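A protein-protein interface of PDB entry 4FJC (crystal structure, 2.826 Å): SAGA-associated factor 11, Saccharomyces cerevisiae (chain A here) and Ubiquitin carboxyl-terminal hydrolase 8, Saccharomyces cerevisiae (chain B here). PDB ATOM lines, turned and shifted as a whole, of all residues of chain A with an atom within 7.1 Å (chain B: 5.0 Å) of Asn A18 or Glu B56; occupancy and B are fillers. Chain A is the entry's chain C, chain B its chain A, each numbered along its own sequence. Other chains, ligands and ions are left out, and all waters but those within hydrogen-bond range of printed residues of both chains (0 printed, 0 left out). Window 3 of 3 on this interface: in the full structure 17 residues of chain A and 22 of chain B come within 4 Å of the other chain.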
ATOM      1  N   ASN A  13     -12.179   1.903   2.302  1.00  0.00           N
ATOM      2  CA  ASN A  13     -13.132   2.616   3.136  1.00  0.00           C
ATOM      3  C   ASN A  13     -12.377   3.650   3.965  1.00  0.00           C
ATOM      4  O   ASN A  13     -12.911   4.694   4.303  1.00  0.00           O
ATOM      5  CB  ASN A  13     -13.908   1.639   4.039  1.00  0.00           C
ATOM      6  CG  ASN A  13     -15.061   0.919   3.317  1.00  0.00           C
ATOM      7  OD1 ASN A  13     -15.905   1.538   2.672  1.00  0.00           O
ATOM      8  ND2 ASN A  13     -15.124  -0.391   3.475  1.00  0.00           N
ATOM      9  N   GLY A  14     -11.115   3.381   4.260  1.00  0.00           N
ATOM     10  CA  GLY A  14     -10.272   4.361   4.932  1.00  0.00           C
ATOM     11  C   GLY A  14     -10.015   5.585   4.083  1.00  0.00           C
ATOM     12  O   GLY A  14     -10.044   6.705   4.553  1.00  0.00           O
ATOM     13  N   ILE A  15      -9.765   5.368   2.812  1.00  0.00           N
ATOM     14  CA  ILE A  15      -9.514   6.466   1.920  1.00  0.00           C
ATOM     15  C   ILE A  15     -10.794   7.286   1.686  1.00  0.00           C
ATOM     16  O   ILE A  15     -10.750   8.534   1.610  1.00  0.00           O
ATOM     17  CB  ILE A  15      -8.948   5.942   0.610  1.00  0.00           C
ATOM     18  CG1 ILE A  15      -7.602   5.285   0.880  1.00  0.00           C
ATOM     19  CG2 ILE A  15      -8.764   7.078  -0.356  1.00  0.00           C
ATOM     20  CD1 ILE A  15      -7.107   4.421  -0.245  1.00  0.00           C
ATOM     21  N   LEU A  16     -11.929   6.590   1.599  1.00  0.00           N
ATOM     22  CA  LEU A  16     -13.228   7.265   1.432  1.00  0.00           C
ATOM     23  C   LEU A  16     -13.627   8.108   2.637  1.00  0.00           C
ATOM     24  O   LEU A  16     -14.220   9.175   2.470  1.00  0.00           O
ATOM     25  CB  LEU A  16     -14.363   6.276   1.125  1.00  0.00           C
ATOM     26  CG  LEU A  16     -15.713   6.996   0.913  1.00  0.00           C
ATOM     27  CD1 LEU A  16     -15.610   8.067  -0.159  1.00  0.00           C
ATOM     28  CD2 LEU A  16     -16.837   6.029   0.591  1.00  0.00           C
ATOM     29  N   ASN A  17     -13.319   7.618   3.839  1.00  0.00           N
ATOM     30  CA  ASN A  17     -13.702   8.292   5.081  1.00  0.00           C
ATOM     31  C   ASN A  17     -12.876   9.560   5.328  1.00  0.00           C
ATOM     32  O   ASN A  17     -13.371  10.624   5.660  1.00  0.00           O
ATOM     33  CB  ASN A  17     -13.508   7.329   6.212  1.00  0.00           C
ATOM     34  CG  ASN A  17     -13.904   7.909   7.521  1.00  0.00           C
ATOM     35  OD1 ASN A  17     -15.076   8.107   7.782  1.00  0.00           O
ATOM     36  ND2 ASN A  17     -12.933   8.170   8.364  1.00  0.00           N
ATOM     37  N   ASN A  18     -11.584   9.410   5.155  1.00  0.00           N
ATOM     38  CA  ASN A  18     -10.694  10.525   5.013  1.00  0.00           C
ATOM     39  C   ASN A  18     -11.202  11.605   4.032  1.00  0.00           C
ATOM     40  O   ASN A  18     -11.155  12.802   4.346  1.00  0.00           O
ATOM     41  CB  ASN A  18      -9.362  10.003   4.524  1.00  0.00           C
ATOM     42  CG  ASN A  18      -8.464   9.576   5.646  1.00  0.00           C
ATOM     43  OD1 ASN A  18      -7.276   9.922   5.650  1.00  0.00           O
ATOM     44  ND2 ASN A  18      -9.001   8.813   6.593  1.00  0.00           N
ATOM     45  N   LEU A  19     -11.656  11.197   2.849  1.00  0.00           N
ATOM     46  CA  LEU A  19     -12.085  12.172   1.883  1.00  0.00           C
ATOM     47  C   LEU A  19     -13.353  12.769   2.376  1.00  0.00           C
ATOM     48  O   LEU A  19     -13.579  13.951   2.214  1.00  0.00           O
ATOM     49  CB  LEU A  19     -12.294  11.580   0.486  1.00  0.00           C
ATOM     50  CG  LEU A  19     -11.057  11.336  -0.368  1.00  0.00           C
ATOM     51  CD1 LEU A  19     -11.429  10.544  -1.600  1.00  0.00           C
ATOM     52  CD2 LEU A  19     -10.380  12.634  -0.751  1.00  0.00           C
ATOM     53  N   LEU A  20     -14.196  11.961   2.988  1.00  0.00           N
ATOM     54  CA  LEU A  20     -15.530  12.438   3.335  1.00  0.00           C
ATOM     55  C   LEU A  20     -15.526  13.338   4.570  1.00  0.00           C
ATOM     56  O   LEU A  20     -16.248  14.320   4.619  1.00  0.00           O
ATOM     57  CB  LEU A  20     -16.464  11.254   3.571  1.00  0.00           C
ATOM     58  CG  LEU A  20     -17.063  10.529   2.362  1.00  0.00           C
ATOM     59  CD1 LEU A  20     -17.841   9.318   2.895  1.00  0.00           C
ATOM     60  CD2 LEU A  20     -17.933  11.462   1.528  1.00  0.00           C
ATOM     61  N   THR A  21     -14.736  12.963   5.577  1.00  0.00           N
ATOM     62  CA  THR A  21     -14.582  13.749   6.799  1.00  0.00           C
ATOM     63  C   THR A  21     -13.892  15.108   6.517  1.00  0.00           C
ATOM     64  O   THR A  21     -14.190  16.095   7.189  1.00  0.00           O
ATOM     65  CB  THR A  21     -13.806  12.957   7.892  1.00  0.00           C
ATOM     66  OG1 THR A  21     -12.583  12.446   7.356  1.00  0.00           O
ATOM     67  CG2 THR A  21     -14.646  11.792   8.417  1.00  0.00           C
ATOM     68  N   THR A  22     -12.996  15.178   5.530  1.00  0.00           N
ATOM     69  CA  THR A  22     -12.378  16.456   5.198  1.00  0.00           C
ATOM     70  C   THR A  22     -13.438  17.400   4.640  1.00  0.00           C
ATOM     71  O   THR A  22     -13.519  18.565   5.029  1.00  0.00           O
ATOM     72  CB  THR A  22     -11.218  16.339   4.182  1.00  0.00           C
ATOM     73  OG1 THR A  22     -10.169  15.519   4.721  1.00  0.00           O
ATOM     74  CG2 THR A  22     -10.652  17.717   3.863  1.00  0.00           C
ATOM     75  N   LEU A  23     -14.266  16.891   3.749  1.00  0.00           N
ATOM     76  CA  LEU A  23     -15.250  17.712   3.070  1.00  0.00           C
ATOM     77  C   LEU A  23     -16.286  18.229   4.069  1.00  0.00           C
ATOM     78  O   LEU A  23     -16.754  19.383   3.973  1.00  0.00           O
ATOM     79  CB  LEU A  23     -15.939  16.904   1.980  1.00  0.00           C
ATOM     80  CG  LEU A  23     -16.198  17.591   0.645  1.00  0.00           C
ATOM     81  CD1 LEU A  23     -17.012  16.673  -0.260  1.00  0.00           C
ATOM     82  CD2 LEU A  23     -16.895  18.923   0.843  1.00  0.00           C
ATOM     83  N   GLN A  25     -15.812  18.677   7.233  1.00  0.00           N
ATOM     84  CA  GLN A  25     -15.216  19.579   8.173  1.00  0.00           C
ATOM     85  C   GLN A  25     -14.923  20.938   7.512  1.00  0.00           C
ATOM     86  O   GLN A  25     -14.841  21.953   8.198  1.00  0.00           O
ATOM     87  CB  GLN A  25     -13.971  18.967   8.780  1.00  0.00           C
ATOM     88  CG  GLN A  25     -14.260  17.879   9.780  1.00  0.00           C
ATOM     89  CD  GLN A  25     -13.022  17.073  10.107  1.00  0.00           C
ATOM     90  OE1 GLN A  25     -13.073  15.843  10.233  1.00  0.00           O
ATOM     91  NE2 GLN A  25     -11.897  17.769  10.273  1.00  0.00           N
ATOM     92  N   MET B  49      -1.791  19.149   3.088  1.00  0.00           N
ATOM     93  CA  MET B  49      -2.835  18.229   3.541  1.00  0.00           C
ATOM     94  C   MET B  49      -2.254  16.885   3.936  1.00  0.00           C
ATOM     95  O   MET B  49      -2.918  15.878   3.816  1.00  0.00           O
ATOM     96  CB  MET B  49      -3.903  18.050   2.449  1.00  0.00           C
ATOM     97  CG  MET B  49      -4.726  19.306   2.245  1.00  0.00           C
ATOM     98  SD  MET B  49      -5.742  19.379   0.772  1.00  0.00           S
ATOM     99  CE  MET B  49      -6.044  21.144   0.742  1.00  0.00           C
ATOM    100  N   LYS B  50      -1.014  16.874   4.412  1.00  0.00           N
ATOM    101  CA  LYS B  50      -0.399  15.654   4.897  1.00  0.00           C
ATOM    102  C   LYS B  50       0.144  15.833   6.289  1.00  0.00           C
ATOM    103  O   LYS B  50       1.058  16.612   6.521  1.00  0.00           O
ATOM    104  CB  LYS B  50       0.749  15.220   4.014  1.00  0.00           C
ATOM    105  CG  LYS B  50       1.093  13.762   4.222  1.00  0.00           C
ATOM    106  CD  LYS B  50       2.558  13.525   4.391  1.00  0.00           C
ATOM    107  CE  LYS B  50       3.319  13.810   3.127  1.00  0.00           C
ATOM    108  NZ  LYS B  50       4.615  13.106   3.344  1.00  0.00           N
ATOM    109  N   CYS B  51      -0.402  15.074   7.218  1.00  0.00           N
ATOM    110  CA  CYS B  51      -0.011  15.209   8.623  1.00  0.00           C
ATOM    111  C   CYS B  51       1.483  14.921   8.867  1.00  0.00           C
ATOM    112  O   CYS B  51       2.030  13.937   8.388  1.00  0.00           O
ATOM    113  CB  CYS B  51      -0.881  14.293   9.470  1.00  0.00           C
ATOM    114  SG  CYS B  51      -0.596  14.435  11.209  1.00  0.00           S
ATOM    115  N   CYS B  54       1.207  11.489  11.367  1.00  0.00           N
ATOM    116  CA  CYS B  54       0.796  10.214  10.758  1.00  0.00           C
ATOM    117  C   CYS B  54       0.971  10.117   9.247  1.00  0.00           C
ATOM    118  O   CYS B  54       0.662   9.077   8.697  1.00  0.00           O
ATOM    119  CB  CYS B  54      -0.647   9.842  11.117  1.00  0.00           C
ATOM    120  SG  CYS B  54      -1.933  10.963  10.499  1.00  0.00           S
ATOM    121  N   HIS B  55       1.413  11.174   8.566  1.00  0.00           N
ATOM    122  CA  HIS B  55       1.575  11.146   7.084  1.00  0.00           C
ATOM    123  C   HIS B  55       0.368  10.757   6.272  1.00  0.00           C
ATOM    124  O   HIS B  55       0.505  10.467   5.088  1.00  0.00           O
ATOM    125  CB  HIS B  55       2.720  10.223   6.700  1.00  0.00           C
ATOM    126  CG  HIS B  55       3.946  10.418   7.558  1.00  0.00           C
ATOM    127  ND1 HIS B  55       4.341   9.514   8.468  1.00  0.00           N
ATOM    128  CD2 HIS B  55       4.817  11.501   7.669  1.00  0.00           C
ATOM    129  CE1 HIS B  55       5.436   9.979   9.099  1.00  0.00           C
ATOM    130  NE2 HIS B  55       5.713  11.202   8.610  1.00  0.00           N
ATOM    131  N   GLU B  56      -0.823  10.745   6.872  1.00  0.00           N
ATOM    132  CA  GLU B  56      -2.020  10.463   6.101  1.00  0.00           C
ATOM    133  C   GLU B  56      -2.396  11.726   5.361  1.00  0.00           C
ATOM    134  O   GLU B  56      -2.202  12.826   5.882  1.00  0.00           O
ATOM    135  CB  GLU B  56      -3.192  10.051   6.998  1.00  0.00           C
ATOM    136  CG  GLU B  56      -3.276   8.571   7.308  1.00  0.00           C
ATOM    137  CD  GLU B  56      -4.617   8.196   7.909  1.00  0.00           C
ATOM    138  OE1 GLU B  56      -5.658   8.507   7.274  1.00  0.00           O
ATOM    139  OE2 GLU B  56      -4.637   7.594   9.017  1.00  0.00           O
ATOM    140  N   ILE B  57      -2.936  11.572   4.159  1.00  0.00           N
ATOM    141  CA  ILE B  57      -3.500  12.688   3.442  1.00  0.00           C
ATOM    142  C   ILE B  57      -4.964  12.778   3.829  1.00  0.00           C
ATOM    143  O   ILE B  57      -5.679  11.754   3.805  1.00  0.00           O
ATOM    144  CB  ILE B  57      -3.432  12.491   1.926  1.00  0.00           C
ATOM    145  CG1 ILE B  57      -1.990  12.237   1.459  1.00  0.00           C
ATOM    146  CG2 ILE B  57      -4.021  13.693   1.213  1.00  0.00           C
ATOM    147  CD1 ILE B  57      -1.035  13.360   1.758  1.00  0.00           C
ATOM    148  N   ASN B  58      -5.415  13.980   4.176  1.00  0.00           N
ATOM    149  CA  ASN B  58      -6.823  14.242   4.419  1.00  0.00           C
ATOM    150  C   ASN B  58      -7.330  13.400   5.575  1.00  0.00           C
ATOM    151  O   ASN B  58      -8.363  12.752   5.488  1.00  0.00           O
ATOM    152  CB  ASN B  58      -7.682  13.974   3.166  1.00  0.00           C
ATOM    153  CG  ASN B  58      -7.596  15.074   2.124  1.00  0.00           C
ATOM    154  OD1 ASN B  58      -7.345  16.250   2.438  1.00  0.00           O
ATOM    155  ND2 ASN B  58      -7.830  14.698   0.855  1.00  0.00           N
ATOM    156  N   SER B  59      -6.600  13.400   6.673  1.00  0.00           N
ATOM    157  CA  SER B  59      -7.091  12.749   7.873  1.00  0.00           C
ATOM    158  C   SER B  59      -8.021  13.754   8.513  1.00  0.00           C
ATOM    159  O   SER B  59      -7.766  14.263   9.578  1.00  0.00           O
ATOM    160  CB  SER B  59      -5.923  12.371   8.777  1.00  0.00           C
ATOM    161  OG  SER B  59      -6.378  11.857  10.008  1.00  0.00           O
ATOM    162  N   GLY B  60      -9.108  14.053   7.823  1.00  0.00           N
ATOM    163  CA  GLY B  60      -9.910  15.226   8.141  1.00  0.00           C
ATOM    164  C   GLY B  60      -9.152  16.495   7.750  1.00  0.00           C
ATOM    165  O   GLY B  60      -8.268  16.452   6.874  1.00  0.00           O
ATOM    166  N   HIS B  76      -6.993  12.602  14.266  1.00  0.00           N
ATOM    167  CA  HIS B  76      -6.163  11.980  15.281  1.00  0.00           C
ATOM    168  C   HIS B  76      -5.576  13.029  16.218  1.00  0.00           C
ATOM    169  O   HIS B  76      -4.652  12.751  16.990  1.00  0.00           O
ATOM    170  CB  HIS B  76      -5.013  11.206  14.650  1.00  0.00           C
ATOM    171  CG  HIS B  76      -5.415  10.161  13.622  1.00  0.00           C
ATOM    172  ND1 HIS B  76      -4.734   9.995  12.464  1.00  0.00           N
ATOM    173  CD2 HIS B  76      -6.407   9.161  13.628  1.00  0.00           C
ATOM    174  CE1 HIS B  76      -5.280   8.963  11.747  1.00  0.00           C
ATOM    175  NE2 HIS B  76      -6.293   8.458  12.456  1.00  0.00           N
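The backbone carbonyl oxygen (O) of Asn B58 lies close to the side-chain hydroxyl (OG1) of Thr A22.
O of Gly B60 sits at hydrogen-bond distance from OG1 of Thr A22 (3.0 Å).
O of Ile B57 sits close to OD1 of Asn A18, at 3.1 Å.
OE1 of Glu B56 lies close to OD1 of Asn A18 (2.7 Å).
The side-chain amide oxygen of Asn A18 lies close to the backbone carbonyl oxygen of Asn B58 (3.0 Å).
Asn A18 touches four residues of chain B.
Glu B56 touches just one residue of chain A: Asn A18 (2.7 Å).
Of the printed residues of chain A, Gly B60 touches Thr A21 (3.9 Å), Thr A22 (3.0 Å) and Gln A25 (3.8 Å).
Of the printed residues of chain B, Thr A21 touches Gly B60 (3.9 Å).
The nearest printed residue of chain A that does not touch Ile B57 is Thr A22 (5.9 Å).
Of the 12 printed residues of chain A, 5 touch a printed residue of chain B.
Hydrophobic or aromatic side chains of chain A within 4 Å of the printed part of chain B: Leu A19.
Along chain A the printed residues that touch a printed residue of chain B span positions 18 to 25.
Among the printed residues, 9 pairs touch across the chains.
The backbone NH (N) of Glu B56 lies close to the side-chain sulfur (SG) of Cys B54.
O of Gly A14 sits at hydrogen-bond distance from ND2 of Asn A18 (3.1 Å).
OE1 of Gln A25 lies close to O of Thr A21 (3.3 Å).
A ring nitrogen (ND1) of His B76 lies within hydrogen-bond range of the side-chain hydroxyl (OG) of Ser B59 (3.5 Å).
O of Asn A18 sits at hydrogen-bond distance from OG1 of Thr A21 (3.4 Å).
The backbone carbonyl oxygen (O) of Glu B56 is in hydrogen-bond range of the backbone NH (N) of Cys B51.
Asn A18 touches Ser B59.
CD2 of Leu A19 touches ND2 of Asn B58 (3.7 Å).
Thr A21 touches Gly B60.
Gln A25 touches Gly B60 (OE1 to CA, 3.8 Å).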
